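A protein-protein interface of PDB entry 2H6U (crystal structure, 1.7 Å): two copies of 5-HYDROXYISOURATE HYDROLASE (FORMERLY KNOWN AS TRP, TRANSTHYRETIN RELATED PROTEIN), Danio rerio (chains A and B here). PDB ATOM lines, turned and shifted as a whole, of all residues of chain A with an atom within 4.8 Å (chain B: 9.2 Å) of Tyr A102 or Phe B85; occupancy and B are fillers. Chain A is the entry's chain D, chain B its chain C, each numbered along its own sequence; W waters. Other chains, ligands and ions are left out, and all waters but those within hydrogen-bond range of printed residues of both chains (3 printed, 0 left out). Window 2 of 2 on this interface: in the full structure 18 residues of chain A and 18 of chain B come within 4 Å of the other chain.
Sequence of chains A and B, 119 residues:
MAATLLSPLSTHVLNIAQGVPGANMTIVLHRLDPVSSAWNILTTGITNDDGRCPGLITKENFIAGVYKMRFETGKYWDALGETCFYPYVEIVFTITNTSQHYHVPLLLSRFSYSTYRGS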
ATOM      1  N   PRO A   8       1.964 -28.832 -25.283  1.00  0.00           N
ATOM      2  CA  PRO A   8       3.155 -28.160 -25.796  1.00  0.00           C
ATOM      3  C   PRO A   8       4.397 -29.055 -25.752  1.00  0.00           C
ATOM      4  O   PRO A   8       5.398 -28.728 -26.380  1.00  0.00           O
ATOM      5  CB  PRO A   8       3.329 -26.976 -24.847  1.00  0.00           C
ATOM      6  CG  PRO A   8       2.681 -27.398 -23.583  1.00  0.00           C
ATOM      7  CD  PRO A   8       1.543 -28.299 -23.977  1.00  0.00           C
ATOM      8  N   LEU A   9       4.319 -30.152 -25.003  1.00  0.00           N
ATOM      9  CA  LEU A   9       5.367 -31.172 -24.980  1.00  0.00           C
ATOM     10  C   LEU A   9       4.863 -32.444 -25.656  1.00  0.00           C
ATOM     11  O   LEU A   9       3.807 -32.979 -25.284  1.00  0.00           O
ATOM     12  CB  LEU A   9       5.758 -31.490 -23.548  1.00  0.00           C
ATOM     13  CG  LEU A   9       6.957 -32.416 -23.332  1.00  0.00           C
ATOM     14  CD1 LEU A   9       8.203 -31.843 -24.082  1.00  0.00           C
ATOM     15  CD2 LEU A   9       7.236 -32.579 -21.861  1.00  0.00           C
ATOM     16  N   SER A  10       5.604 -32.932 -26.655  1.00  0.00           N
ATOM     17  CA  SER A  10       5.252 -34.200 -27.305  1.00  0.00           C
ATOM     18  C   SER A  10       6.456 -35.155 -27.390  1.00  0.00           C
ATOM     19  O   SER A  10       7.585 -34.765 -27.165  1.00  0.00           O
ATOM     20  CB  SER A  10       4.653 -33.976 -28.701  1.00  0.00           C
ATOM     21  OG  SER A  10       5.563 -33.356 -29.578  1.00  0.00           O
ATOM     22  N   PHE A  62       2.965 -25.981 -18.109  1.00  0.00           N
ATOM     23  CA  PHE A  62       4.261 -26.015 -18.785  1.00  0.00           C
ATOM     24  C   PHE A  62       5.053 -24.762 -18.432  1.00  0.00           C
ATOM     25  O   PHE A  62       5.132 -23.818 -19.211  1.00  0.00           O
ATOM     26  CB  PHE A  62       4.061 -26.145 -20.300  1.00  0.00           C
ATOM     27  CG  PHE A  62       5.291 -26.611 -21.053  1.00  0.00           C
ATOM     28  CD1 PHE A  62       6.102 -27.610 -20.536  1.00  0.00           C
ATOM     29  CD2 PHE A  62       5.606 -26.072 -22.298  1.00  0.00           C
ATOM     30  CE1 PHE A  62       7.222 -28.047 -21.232  1.00  0.00           C
ATOM     31  CE2 PHE A  62       6.724 -26.514 -23.004  1.00  0.00           C
ATOM     32  CZ  PHE A  62       7.526 -27.504 -22.466  1.00  0.00           C
ATOM     33  N   VAL A  92      16.859 -35.573 -19.623  1.00  0.00           N
ATOM     34  CA  VAL A  92      16.667 -34.405 -18.757  1.00  0.00           C
ATOM     35  C   VAL A  92      16.878 -33.155 -19.640  1.00  0.00           C
ATOM     36  O   VAL A  92      17.857 -33.076 -20.388  1.00  0.00           O
ATOM     37  CB  VAL A  92      17.641 -34.397 -17.555  1.00  0.00           C
ATOM     38  CG1 VAL A  92      17.486 -33.119 -16.746  1.00  0.00           C
ATOM     39  CG2 VAL A  92      17.432 -35.622 -16.657  1.00  0.00           C
ATOM     40  N   PHE A  93      15.942 -32.218 -19.604  1.00  0.00           N
ATOM     41  CA  PHE A  93      16.034 -31.062 -20.513  1.00  0.00           C
ATOM     42  C   PHE A  93      15.531 -29.775 -19.882  1.00  0.00           C
ATOM     43  O   PHE A  93      14.740 -29.797 -18.928  1.00  0.00           O
ATOM     44  CB  PHE A  93      15.341 -31.319 -21.852  1.00  0.00           C
ATOM     45  CG  PHE A  93      13.900 -31.750 -21.717  1.00  0.00           C
ATOM     46  CD1 PHE A  93      13.574 -33.094 -21.556  1.00  0.00           C
ATOM     47  CD2 PHE A  93      12.880 -30.812 -21.744  1.00  0.00           C
ATOM     48  CE1 PHE A  93      12.249 -33.493 -21.416  1.00  0.00           C
ATOM     49  CE2 PHE A  93      11.526 -31.211 -21.624  1.00  0.00           C
ATOM     50  CZ  PHE A  93      11.224 -32.545 -21.449  1.00  0.00           C
ATOM     51  N   THR A  94      16.024 -28.663 -20.420  1.00  0.00           N
ATOM     52  CA  THR A  94      15.707 -27.337 -19.896  1.00  0.00           C
ATOM     53  C   THR A  94      14.703 -26.627 -20.768  1.00  0.00           C
ATOM     54  O   THR A  94      14.882 -26.480 -21.998  1.00  0.00           O
ATOM     55  CB  THR A  94      16.978 -26.472 -19.724  1.00  0.00           C
ATOM     56  OG1 THR A  94      17.875 -27.153 -18.854  1.00  0.00           O
ATOM     57  CG2 THR A  94      16.643 -25.101 -19.108  1.00  0.00           C
ATOM     58  N   ILE A  95      13.638 -26.184 -20.105  1.00  0.00           N
ATOM     59  CA  ILE A  95      12.620 -25.367 -20.708  1.00  0.00           C
ATOM     60  C   ILE A  95      12.798 -23.961 -20.138  1.00  0.00           C
ATOM     61  O   ILE A  95      12.752 -23.747 -18.910  1.00  0.00           O
ATOM     62  CB  ILE A  95      11.216 -25.927 -20.418  1.00  0.00           C
ATOM     63  CG1 ILE A  95      11.110 -27.372 -20.918  1.00  0.00           C
ATOM     64  CG2 ILE A  95      10.151 -25.079 -21.073  1.00  0.00           C
ATOM     65  CD1 ILE A  95      11.472 -27.528 -22.355  1.00  0.00           C
ATOM     66  N   THR A  96      13.071 -23.026 -21.042  1.00  0.00           N
ATOM     67  CA  THR A  96      13.275 -21.625 -20.689  1.00  0.00           C
ATOM     68  C   THR A  96      12.193 -20.818 -21.386  1.00  0.00           C
ATOM     69  O   THR A  96      11.464 -20.055 -20.753  1.00  0.00           O
ATOM     70  CB  THR A  96      14.680 -21.117 -21.116  1.00  0.00           C
ATOM     71  OG1 THR A  96      15.140 -21.867 -22.246  1.00  0.00           O
ATOM     72  CG2 THR A  96      15.683 -21.289 -19.984  1.00  0.00           C
ATOM     73  N   ASN A  97      12.081 -21.008 -22.693  1.00  0.00           N
ATOM     74  CA  ASN A  97      11.036 -20.348 -23.453  1.00  0.00           C
ATOM     75  C   ASN A  97       9.746 -21.156 -23.519  1.00  0.00           C
ATOM     76  O   ASN A  97       9.561 -21.992 -24.409  1.00  0.00           O
ATOM     77  CB  ASN A  97      11.505 -20.022 -24.861  1.00  0.00           C
ATOM     78  CG  ASN A  97      10.569 -19.072 -25.563  1.00  0.00           C
ATOM     79  OD1 ASN A  97       9.364 -19.070 -25.308  1.00  0.00           O
ATOM     80  ND2 ASN A  97      11.119 -18.238 -26.441  1.00  0.00           N
ATOM     81  N   GLN A 100       7.281 -21.975 -27.032  1.00  0.00           N
ATOM     82  CA  GLN A 100       7.578 -22.827 -28.191  1.00  0.00           C
ATOM     83  C   GLN A 100       7.057 -24.256 -27.972  1.00  0.00           C
ATOM     84  O   GLN A 100       6.772 -24.642 -26.837  1.00  0.00           O
ATOM     85  CB  GLN A 100       9.094 -22.888 -28.435  1.00  0.00           C
ATOM     86  CG  GLN A 100       9.703 -21.607 -28.997  1.00  0.00           C
ATOM     87  CD  GLN A 100      11.206 -21.702 -29.163  1.00  0.00           C
ATOM     88  OE1 GLN A 100      11.748 -22.775 -29.431  1.00  0.00           O
ATOM     89  NE2 GLN A 100      11.892 -20.571 -29.004  1.00  0.00           N
ATOM     90  N   HIS A 101       6.937 -25.031 -29.051  1.00  0.00           N
ATOM     91  CA  HIS A 101       6.642 -26.465 -28.919  1.00  0.00           C
ATOM     92  C   HIS A 101       7.941 -27.259 -28.789  1.00  0.00           C
ATOM     93  O   HIS A 101       8.924 -26.961 -29.467  1.00  0.00           O
ATOM     94  CB  HIS A 101       5.841 -27.004 -30.103  1.00  0.00           C
ATOM     95  CG  HIS A 101       5.311 -28.387 -29.865  1.00  0.00           C
ATOM     96  ND1 HIS A 101       5.973 -29.524 -30.283  1.00  0.00           N
ATOM     97  CD2 HIS A 101       4.221 -28.815 -29.185  1.00  0.00           C
ATOM     98  CE1 HIS A 101       5.294 -30.593 -29.896  1.00  0.00           C
ATOM     99  NE2 HIS A 101       4.230 -30.190 -29.227  1.00  0.00           N
ATOM    100  N   TYR A 102       7.940 -28.258 -27.912  1.00  0.00           N
ATOM    101  CA  TYR A 102       9.110 -29.100 -27.701  1.00  0.00           C
ATOM    102  C   TYR A 102       8.749 -30.556 -27.974  1.00  0.00           C
ATOM    103  O   TYR A 102       7.858 -31.106 -27.344  1.00  0.00           O
ATOM    104  CB  TYR A 102       9.603 -28.958 -26.260  1.00  0.00           C
ATOM    105  CG  TYR A 102      10.202 -27.612 -25.931  1.00  0.00           C
ATOM    106  CD1 TYR A 102      11.582 -27.449 -25.841  1.00  0.00           C
ATOM    107  CD2 TYR A 102       9.393 -26.513 -25.678  1.00  0.00           C
ATOM    108  CE1 TYR A 102      12.135 -26.213 -25.521  1.00  0.00           C
ATOM    109  CE2 TYR A 102       9.930 -25.279 -25.377  1.00  0.00           C
ATOM    110  CZ  TYR A 102      11.300 -25.131 -25.299  1.00  0.00           C
ATOM    111  OH  TYR A 102      11.839 -23.895 -24.974  1.00  0.00           O
ATOM    112  N   HIS A 103       9.452 -31.179 -28.909  1.00  0.00           N
ATOM    113  CA  HIS A 103       9.238 -32.572 -29.231  1.00  0.00           C
ATOM    114  C   HIS A 103      10.503 -33.315 -28.803  1.00  0.00           C
ATOM    115  O   HIS A 103      11.612 -32.961 -29.229  1.00  0.00           O
ATOM    116  CB  HIS A 103       8.978 -32.703 -30.730  1.00  0.00           C
ATOM    117  CG  HIS A 103       8.644 -34.087 -31.180  1.00  0.00           C
ATOM    118  ND1 HIS A 103       9.488 -34.837 -31.975  1.00  0.00           N
ATOM    119  CD2 HIS A 103       7.560 -34.864 -30.945  1.00  0.00           C
ATOM    120  CE1 HIS A 103       8.930 -36.010 -32.219  1.00  0.00           C
ATOM    121  NE2 HIS A 103       7.761 -36.049 -31.604  1.00  0.00           N
ATOM    122  N   VAL A 104      10.335 -34.297 -27.921  1.00  0.00           N
ATOM    123  CA  VAL A 104      11.446 -35.024 -27.305  1.00  0.00           C
ATOM    124  C   VAL A 104      11.249 -36.524 -27.539  1.00  0.00           C
ATOM    125  O   VAL A 104      10.694 -37.223 -26.696  1.00  0.00           O
ATOM    126  CB  VAL A 104      11.502 -34.738 -25.760  1.00  0.00           C
ATOM    127  CG1 VAL A 104      12.598 -35.527 -25.092  1.00  0.00           C
ATOM    128  CG2 VAL A 104      11.671 -33.249 -25.496  1.00  0.00           C
ATOM    129  N   ARG A 117      16.163 -32.422 -29.966  1.00  0.00           N
ATOM    130  CA  ARG A 117      15.104 -31.458 -29.712  1.00  0.00           C
ATOM    131  C   ARG A 117      14.364 -31.131 -30.999  1.00  0.00           C
ATOM    132  O   ARG A 117      14.961 -30.627 -31.956  1.00  0.00           O
ATOM    133  CB  ARG A 117      15.657 -30.200 -29.068  1.00  0.00           C
ATOM    134  CG  ARG A 117      14.578 -29.244 -28.597  1.00  0.00           C
ATOM    135  CD  ARG A 117      14.388 -28.165 -29.641  1.00  0.00           C
ATOM    136  NE  ARG A 117      13.410 -27.164 -29.235  1.00  0.00           N
ATOM    137  CZ  ARG A 117      12.343 -26.851 -29.955  1.00  0.00           C
ATOM    138  NH1 ARG A 117      12.140 -27.465 -31.104  1.00  0.00           N
ATOM    139  NH2 ARG A 117      11.502 -25.918 -29.536  1.00  0.00           N
ATOM    140  N   GLY A 118      13.067 -31.433 -31.026  1.00  0.00           N
ATOM    141  CA  GLY A 118      12.208 -31.073 -32.158  1.00  0.00           C
ATOM    142  C   GLY A 118      11.178 -30.011 -31.810  1.00  0.00           C
ATOM    143  O   GLY A 118      11.069 -29.577 -30.657  1.00  0.00           O
ATOM    144  N   THR B  73      27.141 -32.345 -19.694  1.00  0.00           N
ATOM    145  CA  THR B  73      26.984 -31.695 -21.015  1.00  0.00           C
ATOM    146  C   THR B  73      26.765 -30.167 -20.934  1.00  0.00           C
ATOM    147  O   THR B  73      27.299 -29.377 -21.747  1.00  0.00           O
ATOM    148  CB  THR B  73      25.861 -32.410 -21.823  1.00  0.00           C
ATOM    149  OG1 THR B  73      24.654 -32.396 -21.064  1.00  0.00           O
ATOM    150  CG2 THR B  73      26.227 -33.864 -22.080  1.00  0.00           C
ATOM    151  N   GLY B  74      25.983 -29.719 -19.958  1.00  0.00           N
ATOM    152  CA  GLY B  74      25.661 -28.309 -19.895  1.00  0.00           C
ATOM    153  C   GLY B  74      26.937 -27.559 -19.562  1.00  0.00           C
ATOM    154  O   GLY B  74      27.169 -26.484 -20.089  1.00  0.00           O
ATOM    155  N   TRP B  77      29.293 -27.330 -22.751  1.00  0.00           N
ATOM    156  CA  TRP B  77      28.860 -26.297 -23.709  1.00  0.00           C
ATOM    157  C   TRP B  77      29.016 -24.874 -23.138  1.00  0.00           C
ATOM    158  O   TRP B  77      29.431 -23.943 -23.839  1.00  0.00           O
ATOM    159  CB  TRP B  77      27.423 -26.562 -24.176  1.00  0.00           C
ATOM    160  CG  TRP B  77      27.306 -27.752 -25.097  1.00  0.00           C
ATOM    161  CD1 TRP B  77      26.686 -28.926 -24.830  1.00  0.00           C
ATOM    162  CD2 TRP B  77      27.852 -27.878 -26.423  1.00  0.00           C
ATOM    163  NE1 TRP B  77      26.787 -29.780 -25.908  1.00  0.00           N
ATOM    164  CE2 TRP B  77      27.500 -29.165 -26.897  1.00  0.00           C
ATOM    165  CE3 TRP B  77      28.596 -27.029 -27.252  1.00  0.00           C
ATOM    166  CZ2 TRP B  77      27.880 -29.633 -28.155  1.00  0.00           C
ATOM    167  CZ3 TRP B  77      28.956 -27.494 -28.534  1.00  0.00           C
ATOM    168  CH2 TRP B  77      28.594 -28.784 -28.960  1.00  0.00           C
ATOM    169  N   GLU B  82      28.221 -21.642 -25.087  1.00  0.00           N
ATOM    170  CA  GLU B  82      26.935 -22.003 -25.692  1.00  0.00           C
ATOM    171  C   GLU B  82      25.984 -22.713 -24.727  1.00  0.00           C
ATOM    172  O   GLU B  82      26.420 -23.310 -23.742  1.00  0.00           O
ATOM    173  CB  GLU B  82      27.175 -22.828 -26.953  1.00  0.00           C
ATOM    174  CG  GLU B  82      27.801 -21.947 -28.059  1.00  0.00           C
ATOM    175  CD  GLU B  82      27.887 -22.622 -29.394  1.00  0.00           C
ATOM    176  OE1 GLU B  82      28.829 -23.425 -29.608  1.00  0.00           O
ATOM    177  OE2 GLU B  82      27.023 -22.328 -30.247  1.00  0.00           O
ATOM    178  N   THR B  83      24.685 -22.598 -25.005  1.00  0.00           N
ATOM    179  CA  THR B  83      23.661 -23.288 -24.228  1.00  0.00           C
ATOM    180  C   THR B  83      23.481 -24.718 -24.763  1.00  0.00           C
ATOM    181  O   THR B  83      23.809 -25.013 -25.920  1.00  0.00           O
ATOM    182  CB  THR B  83      22.301 -22.539 -24.295  1.00  0.00           C
ATOM    183  OG1 THR B  83      21.313 -23.243 -23.517  1.00  0.00           O
ATOM    184  CG2 THR B  83      21.811 -22.489 -25.703  1.00  0.00           C
ATOM    185  N   CYS B  84      22.966 -25.600 -23.912  1.00  0.00           N
ATOM    186  CA  CYS B  84      22.641 -26.973 -24.294  1.00  0.00           C
ATOM    187  C   CYS B  84      21.225 -27.280 -23.823  1.00  0.00           C
ATOM    188  O   CYS B  84      20.826 -26.827 -22.746  1.00  0.00           O
ATOM    189  CB  CYS B  84      23.592 -27.958 -23.600  1.00  0.00           C
ATOM    190  SG  CYS B  84      23.418 -29.732 -24.107  1.00  0.00           S
ATOM    191  N   PHE B  85      20.482 -28.060 -24.601  1.00  0.00           N
ATOM    192  CA  PHE B  85      19.106 -28.432 -24.243  1.00  0.00           C
ATOM    193  C   PHE B  85      19.121 -29.345 -23.019  1.00  0.00           C
ATOM    194  O   PHE B  85      18.183 -29.333 -22.216  1.00  0.00           O
ATOM    195  CB  PHE B  85      18.454 -29.144 -25.430  1.00  0.00           C
ATOM    196  CG  PHE B  85      16.983 -29.461 -25.245  1.00  0.00           C
ATOM    197  CD1 PHE B  85      16.073 -28.471 -24.890  1.00  0.00           C
ATOM    198  CD2 PHE B  85      16.511 -30.742 -25.514  1.00  0.00           C
ATOM    199  CE1 PHE B  85      14.703 -28.774 -24.750  1.00  0.00           C
ATOM    200  CE2 PHE B  85      15.161 -31.060 -25.383  1.00  0.00           C
ATOM    201  CZ  PHE B  85      14.250 -30.067 -25.010  1.00  0.00           C
ATOM    202  N   TYR B  86      20.183 -30.143 -22.891  1.00  0.00           N
ATOM    203  CA  TYR B  86      20.335 -31.112 -21.796  1.00  0.00           C
ATOM    204  C   TYR B  86      21.353 -30.584 -20.782  1.00  0.00           C
ATOM    205  O   TYR B  86      22.526 -30.436 -21.120  1.00  0.00           O
ATOM    206  CB  TYR B  86      20.815 -32.468 -22.366  1.00  0.00           C
ATOM    207  CG  TYR B  86      20.091 -32.860 -23.649  1.00  0.00           C
ATOM    208  CD1 TYR B  86      18.827 -33.439 -23.613  1.00  0.00           C
ATOM    209  CD2 TYR B  86      20.672 -32.632 -24.896  1.00  0.00           C
ATOM    210  CE1 TYR B  86      18.155 -33.789 -24.790  1.00  0.00           C
ATOM    211  CE2 TYR B  86      20.011 -32.942 -26.074  1.00  0.00           C
ATOM    212  CZ  TYR B  86      18.757 -33.539 -26.023  1.00  0.00           C
ATOM    213  OH  TYR B  86      18.104 -33.842 -27.197  1.00  0.00           O
ATOM    214  N   PRO B  87      20.929 -30.328 -19.533  1.00  0.00           N
ATOM    215  CA  PRO B  87      21.936 -29.827 -18.603  1.00  0.00           C
ATOM    216  C   PRO B  87      22.961 -30.892 -18.207  1.00  0.00           C
ATOM    217  O   PRO B  87      24.045 -30.563 -17.798  1.00  0.00           O
ATOM    218  CB  PRO B  87      21.123 -29.411 -17.384  1.00  0.00           C
ATOM    219  CG  PRO B  87      19.905 -30.341 -17.444  1.00  0.00           C
ATOM    220  CD  PRO B  87      19.601 -30.481 -18.901  1.00  0.00           C
ATOM    221  N   TYR B  88      22.578 -32.159 -18.301  1.00  0.00           N
ATOM    222  CA  TYR B  88      23.508 -33.285 -18.166  1.00  0.00           C
ATOM    223  C   TYR B  88      22.854 -34.477 -18.837  1.00  0.00           C
ATOM    224  O   TYR B  88      21.647 -34.457 -19.146  1.00  0.00           O
ATOM    225  CB  TYR B  88      23.828 -33.605 -16.689  1.00  0.00           C
ATOM    226  CG  TYR B  88      22.596 -33.877 -15.841  1.00  0.00           C
ATOM    227  CD1 TYR B  88      21.989 -32.853 -15.123  1.00  0.00           C
ATOM    228  CD2 TYR B  88      22.039 -35.152 -15.777  1.00  0.00           C
ATOM    229  CE1 TYR B  88      20.857 -33.087 -14.364  1.00  0.00           C
ATOM    230  CE2 TYR B  88      20.899 -35.402 -15.001  1.00  0.00           C
ATOM    231  CZ  TYR B  88      20.320 -34.359 -14.305  1.00  0.00           C
ATOM    232  OH  TYR B  88      19.191 -34.587 -13.528  1.00  0.00           O
ATOM    233  N   VAL B  89      23.635 -35.533 -19.061  1.00  0.00           N
ATOM    234  CA  VAL B  89      23.079 -36.742 -19.650  1.00  0.00           C
ATOM    235  C   VAL B  89      23.468 -37.934 -18.784  1.00  0.00           C
ATOM    236  O   VAL B  89      24.635 -38.077 -18.413  1.00  0.00           O
ATOM    237  CB  VAL B  89      23.649 -36.963 -21.058  1.00  0.00           C
ATOM    238  CG1 VAL B  89      23.205 -38.351 -21.614  1.00  0.00           C
ATOM    239  CG2 VAL B  89      23.236 -35.797 -21.982  1.00  0.00           C
ATOM    240  N   LEU B 108      27.316 -36.082 -29.272  1.00  0.00           N
ATOM    241  CA  LEU B 108      26.598 -34.937 -28.705  1.00  0.00           C
ATOM    242  C   LEU B 108      26.608 -33.680 -29.580  1.00  0.00           C
ATOM    243  O   LEU B 108      27.635 -33.327 -30.138  1.00  0.00           O
ATOM    244  CB  LEU B 108      27.286 -34.589 -27.370  1.00  0.00           C
ATOM    245  CG  LEU B 108      26.813 -33.391 -26.558  1.00  0.00           C
ATOM    246  CD1 LEU B 108      25.422 -33.727 -25.973  1.00  0.00           C
ATOM    247  CD2 LEU B 108      27.785 -33.018 -25.470  1.00  0.00           C
ATOM    248  N   SER B 109      25.455 -33.019 -29.710  1.00  0.00           N
ATOM    249  CA  SER B 109      25.393 -31.619 -30.152  1.00  0.00           C
ATOM    250  C   SER B 109      24.701 -30.802 -29.056  1.00  0.00           C
ATOM    251  O   SER B 109      24.391 -31.330 -27.970  1.00  0.00           O
ATOM    252  CB  SER B 109      24.657 -31.469 -31.496  1.00  0.00           C
ATOM    253  OG  SER B 109      23.264 -31.736 -31.327  1.00  0.00           O
ATOM    254  N   ARG B 110      24.440 -29.525 -29.315  1.00  0.00           N
ATOM    255  CA  ARG B 110      23.715 -28.725 -28.323  1.00  0.00           C
ATOM    256  C   ARG B 110      22.254 -29.156 -28.177  1.00  0.00           C
ATOM    257  O   ARG B 110      21.620 -28.868 -27.154  1.00  0.00           O
ATOM    258  CB  ARG B 110      23.809 -27.256 -28.672  1.00  0.00           C
ATOM    259  CG  ARG B 110      25.245 -26.802 -28.644  1.00  0.00           C
ATOM    260  CD  ARG B 110      25.315 -25.345 -28.447  1.00  0.00           C
ATOM    261  NE  ARG B 110      24.809 -24.633 -29.588  1.00  0.00           N
ATOM    262  CZ  ARG B 110      23.807 -23.759 -29.555  1.00  0.00           C
ATOM    263  NH1 ARG B 110      23.188 -23.467 -28.429  1.00  0.00           N
ATOM    264  NH2 ARG B 110      23.428 -23.172 -30.674  1.00  0.00           N
ATOM    265  N   PHE B 111      21.743 -29.845 -29.198  1.00  0.00           N
ATOM    266  CA  PHE B 111      20.311 -30.216 -29.235  1.00  0.00           C
ATOM    267  C   PHE B 111      20.047 -31.672 -29.629  1.00  0.00           C
ATOM    268  O   PHE B 111      18.968 -31.990 -30.122  1.00  0.00           O
ATOM    269  CB  PHE B 111      19.547 -29.270 -30.160  1.00  0.00           C
ATOM    270  CG  PHE B 111      19.660 -27.819 -29.776  1.00  0.00           C
ATOM    271  CD1 PHE B 111      18.817 -27.278 -28.810  1.00  0.00           C
ATOM    272  CD2 PHE B 111      20.592 -26.994 -30.387  1.00  0.00           C
ATOM    273  CE1 PHE B 111      18.907 -25.944 -28.444  1.00  0.00           C
ATOM    274  CE2 PHE B 111      20.690 -25.640 -30.024  1.00  0.00           C
ATOM    275  CZ  PHE B 111      19.839 -25.130 -29.044  1.00  0.00           C
ATOM    276  N   SER B 112      21.023 -32.559 -29.401  1.00  0.00           N
ATOM    277  CA  SER B 112      20.853 -33.973 -29.654  1.00  0.00           C
ATOM    278  C   SER B 112      21.925 -34.767 -28.944  1.00  0.00           C
ATOM    279  O   SER B 112      22.995 -34.248 -28.639  1.00  0.00           O
ATOM    280  CB  SER B 112      20.964 -34.298 -31.148  1.00  0.00           C
ATOM    281  OG  SER B 112      22.307 -34.087 -31.604  1.00  0.00           O
ATOM    282  N   TYR B 113      21.626 -36.029 -28.680  1.00  0.00           N
ATOM    283  CA  TYR B 113      22.673 -36.962 -28.335  1.00  0.00           C
ATOM    284  C   TYR B 113      22.278 -38.393 -28.660  1.00  0.00           C
ATOM    285  O   TYR B 113      21.095 -38.709 -28.863  1.00  0.00           O
ATOM    286  CB  TYR B 113      23.106 -36.799 -26.869  1.00  0.00           C
ATOM    287  CG  TYR B 113      22.106 -37.243 -25.810  1.00  0.00           C
ATOM    288  CD1 TYR B 113      21.216 -36.326 -25.241  1.00  0.00           C
ATOM    289  CD2 TYR B 113      22.086 -38.564 -25.349  1.00  0.00           C
ATOM    290  CE1 TYR B 113      20.340 -36.700 -24.252  1.00  0.00           C
ATOM    291  CE2 TYR B 113      21.192 -38.958 -24.350  1.00  0.00           C
ATOM    292  CZ  TYR B 113      20.326 -38.006 -23.809  1.00  0.00           C
ATOM    293  OH  TYR B 113      19.425 -38.368 -22.815  1.00  0.00           O
HETATM  294  O   HOH W   1      19.621 -36.062 -20.440  1.00  0.00           O
HETATM  295  O   HOH W   2      20.265 -27.198 -20.026  1.00  0.00           O
HETATM  296  O   HOH W   3      17.597 -30.947 -32.743  1.00  0.00           O
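O of Phe B111 lies within hydrogen-bond range of N of Arg A117, 2.8 Å away.
The backbone carbonyl oxygen of Phe B85 lies within hydrogen-bond range of the backbone NH of Thr A94 (2.9 Å).
The backbone NH (N) of Phe B85 sits at hydrogen-bond distance from the backbone carbonyl oxygen (O) of Arg B110, 2.9 Å away.
The backbone NH of Phe B111 lies close to the side-chain hydroxyl of Ser B109 (3.2 Å).
NH2 of Arg A117 is in hydrogen-bond range of O of His A101, at 2.8 Å.
The side-chain amide oxygen (OE1) of Gln A100 is in hydrogen-bond range of the guanidinium group (NH2) of Arg A117 (3.2 Å).
OG1 of Thr B73 sits at hydrogen-bond distance from O of Tyr B86.
The backbone NH of Ser A10 sits at hydrogen-bond distance from the backbone carbonyl oxygen of Tyr A102 (3.0 Å).
Among the printed residues, merely in contact across the chains: Val A92 with Tyr B86, Val A92 with Pro B87, Val A92 with Tyr B88, Phe A93 with Phe B85, Phe A93 with Pro B87, Thr A94 with Pro B87, Tyr A102 with Phe B85, Arg A117 with Phe B85 and Arg A117 with Tyr B86.
Of chain B, only Phe B85 comes within 4 Å of Tyr A102.
Of chain A, only Phe A93, Thr A94, Tyr A102 and Arg A117 come within 4 Å of Phe B85.
No residue of chain B comes within 4 Å of Ser A10.
Printed residues of chain B within 4 Å of Arg A117: Phe B85 (3.7 Å), Tyr B86 (3.7 Å) and Phe B111 (2.8 Å).
Of the printed residues of chain A, Phe B111 touches Arg A117 (2.8 Å).
Of the printed residues of chain A, Tyr B86 touches Val A92 (3.4 Å) and Arg A117 (3.7 Å).
Thr A96 touches none of the printed residues of chain B.
The nearest residue of chain B that does not touch Tyr A102 is Phe B111 (7.4 Å).
Of the 17 printed residues of chain A, 5 touch a printed residue of chain B.
Hydrophobic or aromatic side chains of chain A that line the printed part of chain B: Val A92, Phe A93 and Tyr A102.
Of the 17 printed residues of chain B, 5 touch a printed residue of chain A.
Hydrophobic or aromatic side chains of chain B that line the printed part of chain A: Phe B85, Tyr B86, Pro B87 and Tyr B88.
Among the printed residues, 11 pairs touch across the chains.
No position is printed for both chains.
Water W2 bridges OG1 of Thr A94 (2.7 Å) and O of Cys B84 (2.8 Å).
Water W3 bridges O of Arg A117 (2.8 Å) and O of Phe B111 (3.1 Å).
Water W1 lies within hydrogen-bond range of the backbone carbonyl oxygen (O) of Tyr B88, the backbone NH (N) of Val A92 and the side-chain hydroxyl (OH) of Tyr B113.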
